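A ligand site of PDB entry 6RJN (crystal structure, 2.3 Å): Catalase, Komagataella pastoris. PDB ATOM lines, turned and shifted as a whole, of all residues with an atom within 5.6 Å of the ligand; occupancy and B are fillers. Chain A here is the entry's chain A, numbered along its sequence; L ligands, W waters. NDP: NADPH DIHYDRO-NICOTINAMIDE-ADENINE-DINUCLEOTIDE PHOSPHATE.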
ATOM      1  N   PRO A 144     -14.208   6.885 -16.814  1.00  0.00           N
ATOM      2  CA  PRO A 144     -13.829   8.211 -16.305  1.00  0.00           C
ATOM      3  C   PRO A 144     -12.525   8.250 -15.525  1.00  0.00           C
ATOM      4  O   PRO A 144     -12.227   9.290 -14.932  1.00  0.00           O
ATOM      5  CB  PRO A 144     -14.990   8.551 -15.375  1.00  0.00           C
ATOM      6  CG  PRO A 144     -15.302   7.223 -14.741  1.00  0.00           C
ATOM      7  CD  PRO A 144     -15.080   6.171 -15.855  1.00  0.00           C
ATOM      8  N   ILE A 145     -11.758   7.163 -15.492  1.00  0.00           N
ATOM      9  CA  ILE A 145     -10.511   7.089 -14.761  1.00  0.00           C
ATOM     10  C   ILE A 145      -9.503   6.309 -15.598  1.00  0.00           C
ATOM     11  O   ILE A 145      -9.819   5.859 -16.700  1.00  0.00           O
ATOM     12  CB  ILE A 145     -10.697   6.447 -13.385  1.00  0.00           C
ATOM     13  CG1 ILE A 145     -11.411   5.105 -13.539  1.00  0.00           C
ATOM     14  CG2 ILE A 145     -11.482   7.397 -12.509  1.00  0.00           C
ATOM     15  CD1 ILE A 145     -11.607   4.384 -12.283  1.00  0.00           C
ATOM     16  N   HIS A 187      -8.498   1.479  -8.983  1.00  0.00           N
ATOM     17  CA  HIS A 187      -9.815   2.002  -9.352  1.00  0.00           C
ATOM     18  C   HIS A 187     -10.179   1.608 -10.796  1.00  0.00           C
ATOM     19  O   HIS A 187     -11.258   1.063 -11.043  1.00  0.00           O
ATOM     20  CB  HIS A 187      -9.890   3.512  -9.169  1.00  0.00           C
ATOM     21  CG  HIS A 187     -11.291   4.039  -9.140  1.00  0.00           C
ATOM     22  ND1 HIS A 187     -11.578   5.382  -9.024  1.00  0.00           N
ATOM     23  CD2 HIS A 187     -12.480   3.412  -9.223  1.00  0.00           C
ATOM     24  CE1 HIS A 187     -12.896   5.558  -9.049  1.00  0.00           C
ATOM     25  NE2 HIS A 187     -13.463   4.375  -9.158  1.00  0.00           N
ATOM     26  N   TYR A 191     -13.016  -1.095 -12.683  1.00  0.00           N
ATOM     27  CA  TYR A 191     -13.901  -0.716 -13.784  1.00  0.00           C
ATOM     28  C   TYR A 191     -13.633  -1.610 -14.995  1.00  0.00           C
ATOM     29  O   TYR A 191     -14.558  -2.053 -15.678  1.00  0.00           O
ATOM     30  CB  TYR A 191     -13.698   0.755 -14.113  1.00  0.00           C
ATOM     31  CG  TYR A 191     -14.680   1.402 -15.040  1.00  0.00           C
ATOM     32  CD1 TYR A 191     -14.592   1.240 -16.419  1.00  0.00           C
ATOM     33  CD2 TYR A 191     -15.653   2.242 -14.552  1.00  0.00           C
ATOM     34  CE1 TYR A 191     -15.485   1.864 -17.287  1.00  0.00           C
ATOM     35  CE2 TYR A 191     -16.566   2.865 -15.377  1.00  0.00           C
ATOM     36  CZ  TYR A 191     -16.471   2.681 -16.756  1.00  0.00           C
ATOM     37  OH  TYR A 191     -17.368   3.308 -17.600  1.00  0.00           O
ATOM     38  N   SER A 194     -15.242  -5.050 -14.307  1.00  0.00           N
ATOM     39  CA  SER A 194     -16.688  -5.103 -14.411  1.00  0.00           C
ATOM     40  C   SER A 194     -17.065  -5.509 -15.846  1.00  0.00           C
ATOM     41  O   SER A 194     -16.221  -5.628 -16.738  1.00  0.00           O
ATOM     42  CB  SER A 194     -17.289  -3.749 -14.064  1.00  0.00           C
ATOM     43  OG  SER A 194     -17.283  -2.863 -15.190  1.00  0.00           O
ATOM     44  N   ASP A 195     -18.356  -5.662 -16.082  1.00  0.00           N
ATOM     45  CA  ASP A 195     -18.752  -6.014 -17.436  1.00  0.00           C
ATOM     46  C   ASP A 195     -18.646  -4.848 -18.420  1.00  0.00           C
ATOM     47  O   ASP A 195     -18.808  -5.052 -19.626  1.00  0.00           O
ATOM     48  CB  ASP A 195     -20.168  -6.616 -17.422  1.00  0.00           C
ATOM     49  CG  ASP A 195     -20.207  -8.060 -16.853  1.00  0.00           C
ATOM     50  OD1 ASP A 195     -19.168  -8.804 -16.925  1.00  0.00           O
ATOM     51  OD2 ASP A 195     -21.269  -8.439 -16.322  1.00  0.00           O
ATOM     52  N   ARG A 196     -18.328  -3.630 -17.936  1.00  0.00           N
ATOM     53  CA  ARG A 196     -18.071  -2.522 -18.841  1.00  0.00           C
ATOM     54  C   ARG A 196     -16.775  -2.707 -19.599  1.00  0.00           C
ATOM     55  O   ARG A 196     -16.569  -2.064 -20.637  1.00  0.00           O
ATOM     56  CB  ARG A 196     -18.055  -1.203 -18.087  1.00  0.00           C
ATOM     57  CG  ARG A 196     -19.443  -0.633 -17.890  1.00  0.00           C
ATOM     58  CD  ARG A 196     -19.331   0.741 -17.290  1.00  0.00           C
ATOM     59  NE  ARG A 196     -20.638   1.214 -16.841  1.00  0.00           N
ATOM     60  CZ  ARG A 196     -21.008   2.491 -16.867  1.00  0.00           C
ATOM     61  NH1 ARG A 196     -20.187   3.420 -17.333  1.00  0.00           N
ATOM     62  NH2 ARG A 196     -22.219   2.837 -16.439  1.00  0.00           N
ATOM     63  N   ASN A 206     -20.416   4.681 -22.933  1.00  0.00           N
ATOM     64  CA  ASN A 206     -20.224   6.105 -22.702  1.00  0.00           C
ATOM     65  C   ASN A 206     -18.788   6.526 -23.051  1.00  0.00           C
ATOM     66  O   ASN A 206     -17.898   5.698 -23.254  1.00  0.00           O
ATOM     67  CB  ASN A 206     -20.546   6.440 -21.252  1.00  0.00           C
ATOM     68  CG  ASN A 206     -21.988   6.197 -20.899  1.00  0.00           C
ATOM     69  OD1 ASN A 206     -22.863   6.122 -21.761  1.00  0.00           O
ATOM     70  ND2 ASN A 206     -22.246   6.075 -19.606  1.00  0.00           N
ATOM     71  N   TYR A 208     -15.862   9.584 -21.652  1.00  0.00           N
ATOM     72  CA  TYR A 208     -15.520  10.513 -20.586  1.00  0.00           C
ATOM     73  C   TYR A 208     -14.193  11.196 -20.867  1.00  0.00           C
ATOM     74  O   TYR A 208     -13.225  10.558 -21.287  1.00  0.00           O
ATOM     75  CB  TYR A 208     -15.368   9.773 -19.240  1.00  0.00           C
ATOM     76  CG  TYR A 208     -16.522   8.903 -18.876  1.00  0.00           C
ATOM     77  CD1 TYR A 208     -16.635   7.639 -19.399  1.00  0.00           C
ATOM     78  CD2 TYR A 208     -17.482   9.339 -17.988  1.00  0.00           C
ATOM     79  CE1 TYR A 208     -17.672   6.834 -19.065  1.00  0.00           C
ATOM     80  CE2 TYR A 208     -18.538   8.542 -17.646  1.00  0.00           C
ATOM     81  CZ  TYR A 208     -18.625   7.276 -18.182  1.00  0.00           C
ATOM     82  OH  TYR A 208     -19.691   6.463 -17.856  1.00  0.00           O
ATOM     83  N   HIS A 228     -18.807  14.330 -20.022  1.00  0.00           N
ATOM     84  CA  HIS A 228     -19.469  13.038 -20.061  1.00  0.00           C
ATOM     85  C   HIS A 228     -20.290  12.927 -21.348  1.00  0.00           C
ATOM     86  O   HIS A 228     -21.113  13.794 -21.653  1.00  0.00           O
ATOM     87  CB  HIS A 228     -20.388  12.855 -18.874  1.00  0.00           C
ATOM     88  CG  HIS A 228     -19.693  12.908 -17.563  1.00  0.00           C
ATOM     89  ND1 HIS A 228     -19.516  11.802 -16.769  1.00  0.00           N
ATOM     90  CD2 HIS A 228     -19.163  13.953 -16.882  1.00  0.00           C
ATOM     91  CE1 HIS A 228     -18.885  12.151 -15.664  1.00  0.00           C
ATOM     92  NE2 HIS A 228     -18.660  13.452 -15.703  1.00  0.00           N
ATOM     93  N   LYS A 230     -22.940  10.329 -22.880  1.00  0.00           N
ATOM     94  CA  LYS A 230     -23.719   9.153 -22.495  1.00  0.00           C
ATOM     95  C   LYS A 230     -24.556   8.629 -23.669  1.00  0.00           C
ATOM     96  O   LYS A 230     -25.368   9.345 -24.252  1.00  0.00           O
ATOM     97  CB  LYS A 230     -24.609   9.464 -21.290  1.00  0.00           C
ATOM     98  CG  LYS A 230     -23.858  10.057 -20.094  1.00  0.00           C
ATOM     99  CD  LYS A 230     -24.188   9.405 -18.770  1.00  0.00           C
ATOM    100  CE  LYS A 230     -24.893  10.357 -17.809  1.00  0.00           C
ATOM    101  NZ  LYS A 230     -24.925   9.807 -16.408  1.00  0.00           N
ATOM    102  N   VAL A 235     -25.784   1.937 -21.373  1.00  0.00           N
ATOM    103  CA  VAL A 235     -24.602   1.090 -21.324  1.00  0.00           C
ATOM    104  C   VAL A 235     -25.061  -0.352 -21.321  1.00  0.00           C
ATOM    105  O   VAL A 235     -25.725  -0.787 -20.375  1.00  0.00           O
ATOM    106  CB  VAL A 235     -23.728   1.406 -20.099  1.00  0.00           C
ATOM    107  CG1 VAL A 235     -22.579   0.392 -19.970  1.00  0.00           C
ATOM    108  CG2 VAL A 235     -23.219   2.835 -20.192  1.00  0.00           C
ATOM    109  N   GLN A 275     -19.485  18.353 -15.722  1.00  0.00           N
ATOM    110  CA  GLN A 275     -19.381  18.775 -14.334  1.00  0.00           C
ATOM    111  C   GLN A 275     -18.440  19.975 -14.286  1.00  0.00           C
ATOM    112  O   GLN A 275     -17.535  20.099 -15.113  1.00  0.00           O
ATOM    113  CB  GLN A 275     -18.851  17.664 -13.443  1.00  0.00           C
ATOM    114  CG  GLN A 275     -19.641  16.355 -13.417  1.00  0.00           C
ATOM    115  CD  GLN A 275     -18.865  15.239 -12.736  1.00  0.00           C
ATOM    116  OE1 GLN A 275     -17.852  14.781 -13.244  1.00  0.00           O
ATOM    117  NE2 GLN A 275     -19.320  14.806 -11.567  1.00  0.00           N
ATOM    118  N   VAL A 295     -12.905  10.167  -9.757  1.00  0.00           N
ATOM    119  CA  VAL A 295     -14.035  10.853 -10.360  1.00  0.00           C
ATOM    120  C   VAL A 295     -14.476  11.978  -9.437  1.00  0.00           C
ATOM    121  O   VAL A 295     -14.054  12.076  -8.278  1.00  0.00           O
ATOM    122  CB  VAL A 295     -15.226   9.917 -10.618  1.00  0.00           C
ATOM    123  CG1 VAL A 295     -14.831   8.770 -11.449  1.00  0.00           C
ATOM    124  CG2 VAL A 295     -15.790   9.443  -9.291  1.00  0.00           C
ATOM    125  N   TRP A 296     -15.382  12.807  -9.943  1.00  0.00           N
ATOM    126  CA  TRP A 296     -16.049  13.784  -9.105  1.00  0.00           C
ATOM    127  C   TRP A 296     -17.415  13.215  -8.729  1.00  0.00           C
ATOM    128  O   TRP A 296     -18.225  12.940  -9.632  1.00  0.00           O
ATOM    129  CB  TRP A 296     -16.216  15.096  -9.850  1.00  0.00           C
ATOM    130  CG  TRP A 296     -14.980  15.725 -10.294  1.00  0.00           C
ATOM    131  CD1 TRP A 296     -13.705  15.263 -10.123  1.00  0.00           C
ATOM    132  CD2 TRP A 296     -14.867  16.963 -10.999  1.00  0.00           C
ATOM    133  NE1 TRP A 296     -12.817  16.142 -10.684  1.00  0.00           N
ATOM    134  CE2 TRP A 296     -13.504  17.188 -11.232  1.00  0.00           C
ATOM    135  CE3 TRP A 296     -15.793  17.906 -11.452  1.00  0.00           C
ATOM    136  CZ2 TRP A 296     -13.033  18.327 -11.910  1.00  0.00           C
ATOM    137  CZ3 TRP A 296     -15.342  19.027 -12.118  1.00  0.00           C
ATOM    138  CH2 TRP A 296     -13.964  19.232 -12.334  1.00  0.00           C
ATOM    139  N   PRO A 297     -17.720  13.001  -7.435  1.00  0.00           N
ATOM    140  CA  PRO A 297     -19.012  12.391  -7.078  1.00  0.00           C
ATOM    141  C   PRO A 297     -20.187  13.212  -7.586  1.00  0.00           C
ATOM    142  O   PRO A 297     -20.215  14.444  -7.449  1.00  0.00           O
ATOM    143  CB  PRO A 297     -18.980  12.333  -5.554  1.00  0.00           C
ATOM    144  CG  PRO A 297     -17.467  12.257  -5.221  1.00  0.00           C
ATOM    145  CD  PRO A 297     -16.812  13.113  -6.280  1.00  0.00           C
ATOM    146  N   HIS A 298     -21.159  12.506  -8.169  1.00  0.00           N
ATOM    147  CA  HIS A 298     -22.310  13.169  -8.793  1.00  0.00           C
ATOM    148  C   HIS A 298     -23.123  13.980  -7.786  1.00  0.00           C
ATOM    149  O   HIS A 298     -23.740  14.982  -8.162  1.00  0.00           O
ATOM    150  CB  HIS A 298     -23.257  12.151  -9.464  1.00  0.00           C
ATOM    151  CG  HIS A 298     -22.705  11.490 -10.685  1.00  0.00           C
ATOM    152  ND1 HIS A 298     -22.839  10.137 -10.908  1.00  0.00           N
ATOM    153  CD2 HIS A 298     -22.043  11.987 -11.761  1.00  0.00           C
ATOM    154  CE1 HIS A 298     -22.273   9.827 -12.066  1.00  0.00           C
ATOM    155  NE2 HIS A 298     -21.781  10.929 -12.593  1.00  0.00           N
ATOM    156  N   LYS A 299     -23.197  13.564  -6.514  1.00  0.00           N
ATOM    157  CA  LYS A 299     -24.025  14.335  -5.596  1.00  0.00           C
ATOM    158  C   LYS A 299     -23.428  15.724  -5.380  1.00  0.00           C
ATOM    159  O   LYS A 299     -24.160  16.717  -5.307  1.00  0.00           O
ATOM    160  CB  LYS A 299     -24.183  13.595  -4.256  1.00  0.00           C
ATOM    161  CG  LYS A 299     -25.491  13.962  -3.526  1.00  0.00           C
ATOM    162  CD  LYS A 299     -25.379  14.023  -1.954  1.00  0.00           C
ATOM    163  CE  LYS A 299     -26.138  15.270  -1.360  1.00  0.00           C
ATOM    164  NZ  LYS A 299     -27.017  15.020  -0.140  1.00  0.00           N
ATOM    165  N   GLU A 442     -10.881   4.785  -1.369  1.00  0.00           N
ATOM    166  CA  GLU A 442     -12.289   5.057  -1.060  1.00  0.00           C
ATOM    167  C   GLU A 442     -13.159   4.988  -2.306  1.00  0.00           C
ATOM    168  O   GLU A 442     -14.273   4.499  -2.241  1.00  0.00           O
ATOM    169  CB  GLU A 442     -12.446   6.409  -0.359  1.00  0.00           C
ATOM    170  CG  GLU A 442     -12.314   6.382   1.203  1.00  0.00           C
ATOM    171  CD  GLU A 442     -13.282   5.396   1.915  1.00  0.00           C
ATOM    172  OE1 GLU A 442     -14.441   5.189   1.454  1.00  0.00           O
ATOM    173  OE2 GLU A 442     -12.856   4.844   2.959  1.00  0.00           O
ATOM    174  N   GLN A 443     -12.662   5.460  -3.444  1.00  0.00           N
ATOM    175  CA  GLN A 443     -13.450   5.450  -4.713  1.00  0.00           C
ATOM    176  C   GLN A 443     -13.621   4.013  -5.210  1.00  0.00           C
ATOM    177  O   GLN A 443     -14.677   3.685  -5.696  1.00  0.00           O
ATOM    178  CB  GLN A 443     -12.911   6.469  -5.702  1.00  0.00           C
ATOM    179  CG  GLN A 443     -13.108   7.887  -5.213  1.00  0.00           C
ATOM    180  CD  GLN A 443     -13.111   8.919  -6.318  1.00  0.00           C
ATOM    181  OE1 GLN A 443     -12.830   8.620  -7.450  1.00  0.00           O
ATOM    182  NE2 GLN A 443     -13.421  10.137  -5.964  1.00  0.00           N
ATOM    183  N   PRO A 444     -12.583   3.175  -5.183  1.00  0.00           N
ATOM    184  CA  PRO A 444     -12.725   1.755  -5.427  1.00  0.00           C
ATOM    185  C   PRO A 444     -13.744   1.118  -4.462  1.00  0.00           C
ATOM    186  O   PRO A 444     -14.474   0.312  -4.883  1.00  0.00           O
ATOM    187  CB  PRO A 444     -11.316   1.213  -5.190  1.00  0.00           C
ATOM    188  CG  PRO A 444     -10.435   2.361  -5.554  1.00  0.00           C
ATOM    189  CD  PRO A 444     -11.191   3.579  -5.127  1.00  0.00           C
ATOM    190  N   ALA A 446     -16.269   2.666  -3.142  1.00  0.00           N
ATOM    191  CA  ALA A 446     -17.563   3.178  -3.644  1.00  0.00           C
ATOM    192  C   ALA A 446     -17.986   2.405  -4.891  1.00  0.00           C
ATOM    193  O   ALA A 446     -19.154   2.163  -5.019  1.00  0.00           O
ATOM    194  CB  ALA A 446     -17.485   4.656  -3.890  1.00  0.00           C
ATOM    195  N   LEU A 447     -17.052   2.037  -5.763  1.00  0.00           N
ATOM    196  CA  LEU A 447     -17.365   1.283  -6.998  1.00  0.00           C
ATOM    197  C   LEU A 447     -17.913  -0.095  -6.635  1.00  0.00           C
ATOM    198  O   LEU A 447     -18.829  -0.535  -7.299  1.00  0.00           O
ATOM    199  CB  LEU A 447     -16.126   1.210  -7.897  1.00  0.00           C
ATOM    200  CG  LEU A 447     -16.328   0.572  -9.268  1.00  0.00           C
ATOM    201  CD1 LEU A 447     -17.587   1.058  -9.953  1.00  0.00           C
ATOM    202  CD2 LEU A 447     -15.125   0.808 -10.152  1.00  0.00           C
ATOM    203  N   VAL A 450     -21.388   0.325  -5.792  1.00  0.00           N
ATOM    204  CA  VAL A 450     -22.200   0.590  -6.982  1.00  0.00           C
ATOM    205  C   VAL A 450     -22.501  -0.717  -7.710  1.00  0.00           C
ATOM    206  O   VAL A 450     -23.612  -0.910  -8.219  1.00  0.00           O
ATOM    207  CB  VAL A 450     -21.481   1.600  -7.889  1.00  0.00           C
ATOM    208  CG1 VAL A 450     -22.024   1.529  -9.305  1.00  0.00           C
ATOM    209  CG2 VAL A 450     -21.655   2.991  -7.330  1.00  0.00           C
ATOM    210  N   PHE A 451     -21.505  -1.593  -7.814  1.00  0.00           N
ATOM    211  CA  PHE A 451     -21.729  -2.943  -8.306  1.00  0.00           C
ATOM    212  C   PHE A 451     -22.919  -3.585  -7.581  1.00  0.00           C
ATOM    213  O   PHE A 451     -23.807  -4.171  -8.209  1.00  0.00           O
ATOM    214  CB  PHE A 451     -20.481  -3.806  -8.098  1.00  0.00           C
ATOM    215  CG  PHE A 451     -19.315  -3.500  -9.006  1.00  0.00           C
ATOM    216  CD1 PHE A 451     -19.443  -2.664 -10.106  1.00  0.00           C
ATOM    217  CD2 PHE A 451     -18.075  -4.088  -8.771  1.00  0.00           C
ATOM    218  CE1 PHE A 451     -18.348  -2.411 -10.940  1.00  0.00           C
ATOM    219  CE2 PHE A 451     -16.998  -3.849  -9.605  1.00  0.00           C
ATOM    220  CZ  PHE A 451     -17.141  -3.003 -10.688  1.00  0.00           C
ATOM    221  N   LYS A 453     -25.521  -2.535  -6.265  1.00  0.00           N
ATOM    222  CA  LYS A 453     -26.863  -2.035  -6.485  1.00  0.00           C
ATOM    223  C   LYS A 453     -27.508  -2.697  -7.693  1.00  0.00           C
ATOM    224  O   LYS A 453     -28.709  -2.487  -7.925  1.00  0.00           O
ATOM    225  CB  LYS A 453     -26.844  -0.536  -6.694  1.00  0.00           C
ATOM    226  CG  LYS A 453     -26.466   0.318  -5.491  1.00  0.00           C
ATOM    227  CD  LYS A 453     -26.409   1.775  -5.959  1.00  0.00           C
ATOM    228  CE  LYS A 453     -26.388   2.807  -4.827  1.00  0.00           C
ATOM    229  NZ  LYS A 453     -26.856   4.143  -5.349  1.00  0.00           N
ATOM    230  N   THR A 454     -26.736  -3.457  -8.484  1.00  0.00           N
ATOM    231  CA  THR A 454     -27.272  -4.211  -9.611  1.00  0.00           C
ATOM    232  C   THR A 454     -26.994  -5.691  -9.359  1.00  0.00           C
ATOM    233  O   THR A 454     -25.814  -6.076  -9.219  1.00  0.00           O
ATOM    234  CB  THR A 454     -26.673  -3.788 -10.938  1.00  0.00           C
ATOM    235  OG1 THR A 454     -27.088  -2.455 -11.251  1.00  0.00           O
ATOM    236  CG2 THR A 454     -27.145  -4.747 -12.039  1.00  0.00           C
ATOM    237  N   GLN A 457     -23.589  -7.968 -10.509  1.00  0.00           N
ATOM    238  CA  GLN A 457     -22.397  -7.250 -10.930  1.00  0.00           C
ATOM    239  C   GLN A 457     -21.189  -7.559 -10.040  1.00  0.00           C
ATOM    240  O   GLN A 457     -20.065  -7.691 -10.541  1.00  0.00           O
ATOM    241  CB  GLN A 457     -22.679  -5.751 -10.980  1.00  0.00           C
ATOM    242  CG  GLN A 457     -23.274  -5.272 -12.347  1.00  0.00           C
ATOM    243  CD  GLN A 457     -22.385  -5.643 -13.577  1.00  0.00           C
ATOM    244  OE1 GLN A 457     -21.358  -4.980 -13.855  1.00  0.00           O
ATOM    245  NE2 GLN A 457     -22.774  -6.719 -14.301  1.00  0.00           N
HETATM  246  PA  NDP L   1     -23.363   7.515  -8.383  1.00  0.00           P
HETATM  247  O1A NDP L   1     -24.107   6.338  -7.892  1.00  0.00           O
HETATM  248  O2A NDP L   1     -23.952   8.898  -8.247  1.00  0.00           O
HETATM  249  O5B NDP L   1     -22.991   7.214  -9.951  1.00  0.00           O
HETATM  250  C5B NDP L   1     -22.503   5.887 -10.011  1.00  0.00           C
HETATM  251  C4B NDP L   1     -22.054   5.646 -11.478  1.00  0.00           C
HETATM  252  O4B NDP L   1     -21.358   4.441 -11.653  1.00  0.00           O
HETATM  253  C3B NDP L   1     -23.267   5.560 -12.386  1.00  0.00           C
HETATM  254  O3B NDP L   1     -23.804   6.835 -12.565  1.00  0.00           O
HETATM  255  C2B NDP L   1     -22.580   5.043 -13.679  1.00  0.00           C
HETATM  256  O2B NDP L   1     -21.897   5.994 -14.338  1.00  0.00           O
HETATM  257  C1B NDP L   1     -21.498   4.028 -13.036  1.00  0.00           C
HETATM  258  N9A NDP L   1     -21.871   2.617 -12.990  1.00  0.00           N
HETATM  259  C8A NDP L   1     -23.096   2.030 -12.612  1.00  0.00           C
HETATM  260  N7A NDP L   1     -23.075   0.684 -12.643  1.00  0.00           N
HETATM  261  C5A NDP L   1     -21.766   0.391 -13.024  1.00  0.00           C
HETATM  262  C6A NDP L   1     -21.111  -0.839 -13.233  1.00  0.00           C
HETATM  263  N6A NDP L   1     -21.797  -2.052 -13.057  1.00  0.00           N
HETATM  264  N1A NDP L   1     -19.812  -0.875 -13.617  1.00  0.00           N
HETATM  265  C2A NDP L   1     -19.211   0.372 -13.779  1.00  0.00           C
HETATM  266  N3A NDP L   1     -19.688   1.612 -13.613  1.00  0.00           N
HETATM  267  C4A NDP L   1     -21.000   1.585 -13.226  1.00  0.00           C
HETATM  268  O3  NDP L   1     -22.011   7.365  -7.403  1.00  0.00           O
HETATM  269  PN  NDP L   1     -20.911   8.598  -7.292  1.00  0.00           P
HETATM  270  O1N NDP L   1     -20.878   9.611  -8.368  1.00  0.00           O
HETATM  271  O2N NDP L   1     -20.661   9.021  -5.863  1.00  0.00           O
HETATM  272  O5D NDP L   1     -19.439   7.723  -7.617  1.00  0.00           O
HETATM  273  C5D NDP L   1     -19.450   6.461  -6.959  1.00  0.00           C
HETATM  274  C4D NDP L   1     -18.559   5.488  -7.773  1.00  0.00           C
HETATM  275  O4D NDP L   1     -19.142   5.302  -9.089  1.00  0.00           O
HETATM  276  C3D NDP L   1     -17.175   6.163  -8.048  1.00  0.00           C
HETATM  277  O3D NDP L   1     -16.291   5.895  -6.971  1.00  0.00           O
HETATM  278  C2D NDP L   1     -16.731   5.493  -9.361  1.00  0.00           C
HETATM  279  O2D NDP L   1     -16.038   4.301  -9.167  1.00  0.00           O
HETATM  280  C1D NDP L   1     -18.102   5.153 -10.061  1.00  0.00           C
HETATM  281  N1N NDP L   1     -18.334   6.092 -11.166  1.00  0.00           N
HETATM  282  C2N NDP L   1     -18.447   7.476 -10.972  1.00  0.00           C
HETATM  283  C3N NDP L   1     -18.690   8.318 -12.050  1.00  0.00           C
HETATM  284  C7N NDP L   1     -18.752   9.818 -11.838  1.00  0.00           C
HETATM  285  O7N NDP L   1     -18.403  10.649 -12.711  1.00  0.00           O
HETATM  286  N7N NDP L   1     -19.206  10.319 -10.612  1.00  0.00           N
HETATM  287  C4N NDP L   1     -18.841   7.809 -13.405  1.00  0.00           C
HETATM  288  C5N NDP L   1     -18.616   6.357 -13.500  1.00  0.00           C
HETATM  289  C6N NDP L   1     -18.378   5.592 -12.429  1.00  0.00           C
HETATM  290  P2B NDP L   1     -22.709   6.721 -15.762  1.00  0.00           P
HETATM  291  O1X NDP L   1     -21.564   7.611 -16.135  1.00  0.00           O
HETATM  292  O2X NDP L   1     -23.948   7.377 -15.155  1.00  0.00           O
HETATM  293  O3X NDP L   1     -22.902   5.471 -16.572  1.00  0.00           O
HETATM  294  O   HOH W   1     -21.706  10.098 -15.207  1.00  0.00           O
HETATM  295  O   HOH W   2     -23.004   6.684  -4.319  1.00  0.00           O
HETATM  296  O   HOH W   3     -22.414  10.954  -5.470  1.00  0.00           O
HETATM  297  O   HOH W   4     -25.101   5.231 -18.099  1.00  0.00           O
HETATM  298  O   HOH W   5     -24.634  -0.862 -10.613  1.00  0.00           O
HETATM  299  O   HOH W   6     -18.236   8.423  -3.934  1.00  0.00           O
HETATM  300  O   HOH W   7     -16.406  12.582 -12.684  1.00  0.00           O
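NE2 of His 187 is in hydrogen-bond range of O2D of the ligand (2.6 Å).
O3X of the ligand lies within salt-bridge range of NH2 of Arg 196, 2.7 Å away.
The side-chain hydroxyl (OH) of Tyr 208 lies within hydrogen-bond range of an oxygen (O1X) of the ligand (2.8 Å).
An oxygen (O2X) of the ligand lies within salt-bridge range of the side-chain amino group (NZ) of Lys 230, 2.9 Å away.
The backbone NH (N) of His 298 is in hydrogen-bond range of an oxygen (O1N) of the ligand, 2.9 Å away.
An oxygen (O5B) of the ligand lies within hydrogen-bond range of a ring nitrogen (ND1) of His 298 (3.1 Å).
O of Trp 296 lies within hydrogen-bond range of N7N of the ligand, 3.0 Å away.
The backbone carbonyl oxygen of Gln 443 sits at hydrogen-bond distance from an oxygen (O3D) of the ligand (3.0 Å).
A nitrogen (N6A) of the ligand is in hydrogen-bond range of the side-chain amide oxygen (OE1) of Gln 457 (3.1 Å).
O3X of the ligand is in hydrogen-bond range of ND2 of Asn 206 (3.2 Å).
The backbone NH (N) of Arg 196 is in hydrogen-bond range of the side-chain hydroxyl (OG) of Ser 194, 3.0 Å away.
The side-chain hydroxyl (OH) of Tyr 191 sits at hydrogen-bond distance from the guanidinium group (NH1) of Arg 196, 2.8 Å away.
The side-chain amide nitrogen of Asn 206 is in hydrogen-bond range of the side-chain hydroxyl of Tyr 208 (3.1 Å).
The side-chain amide nitrogen (NE2) of Gln 275 is in hydrogen-bond range of the backbone carbonyl oxygen (O) of Trp 296 (2.9 Å).
OE1 of Gln 443 is in hydrogen-bond range of N of Val 295 (2.8 Å).
The side-chain carboxylate (OD2) of Asp 195 sits at hydrogen-bond distance from the side-chain amide nitrogen (NE2) of Gln 457, 3.1 Å away.
A ring nitrogen (NE2) of His 228 sits at hydrogen-bond distance from the side-chain amide oxygen (OE1) of Gln 275 (2.9 Å).
The side-chain hydroxyl (OG) of Ser 194 lies within hydrogen-bond range of the backbone carbonyl oxygen (O) of Tyr 191.
Pro 144 touches the ligand.
CE2 of Tyr 191 touches N3A of the ligand (3.8 Å).
Ser 194 touches the ligand.
His 228 touches the ligand.
Val 295 touches the ligand.
Pro 297 touches the ligand.
Ala 446 touches the ligand.
Leu 447 touches the ligand.
Val 450 touches the ligand.
Phe 451 touches the ligand (CE1 to N1A, 3.4 Å).
Hydrophobic or aromatic side chains that line the ligand: Pro 144, His 187, Tyr 191, Tyr 208, His 228, Val 295, Pro 297, His 298, Ala 446, Leu 447, Val 450 and Phe 451.
Of the 28 residues printed, 19 come within 4 Å of the ligand.
Water W3 lies within hydrogen-bond range of O2N of the ligand, N of Lys 299 and N of His 298.
Water W1 lies within hydrogen-bond range of O1X of the ligand, NE2 of His 298, ND1 of His 228 and NZ of Lys 230.
Water W4 bridges O3X of the ligand (2.7 Å) and ND2 of Asn 206 (3.3 Å).
Water W7 lies within hydrogen-bond range of the side-chain amide oxygen of Gln 275, an oxygen (O7N) of the ligand and the backbone NH of Trp 296.
Water W5 lies within hydrogen-bond range of O of Val 450 (2.6 Å), N7A of the ligand (3.0 Å) and OG1 of Thr 454 (3.0 Å).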
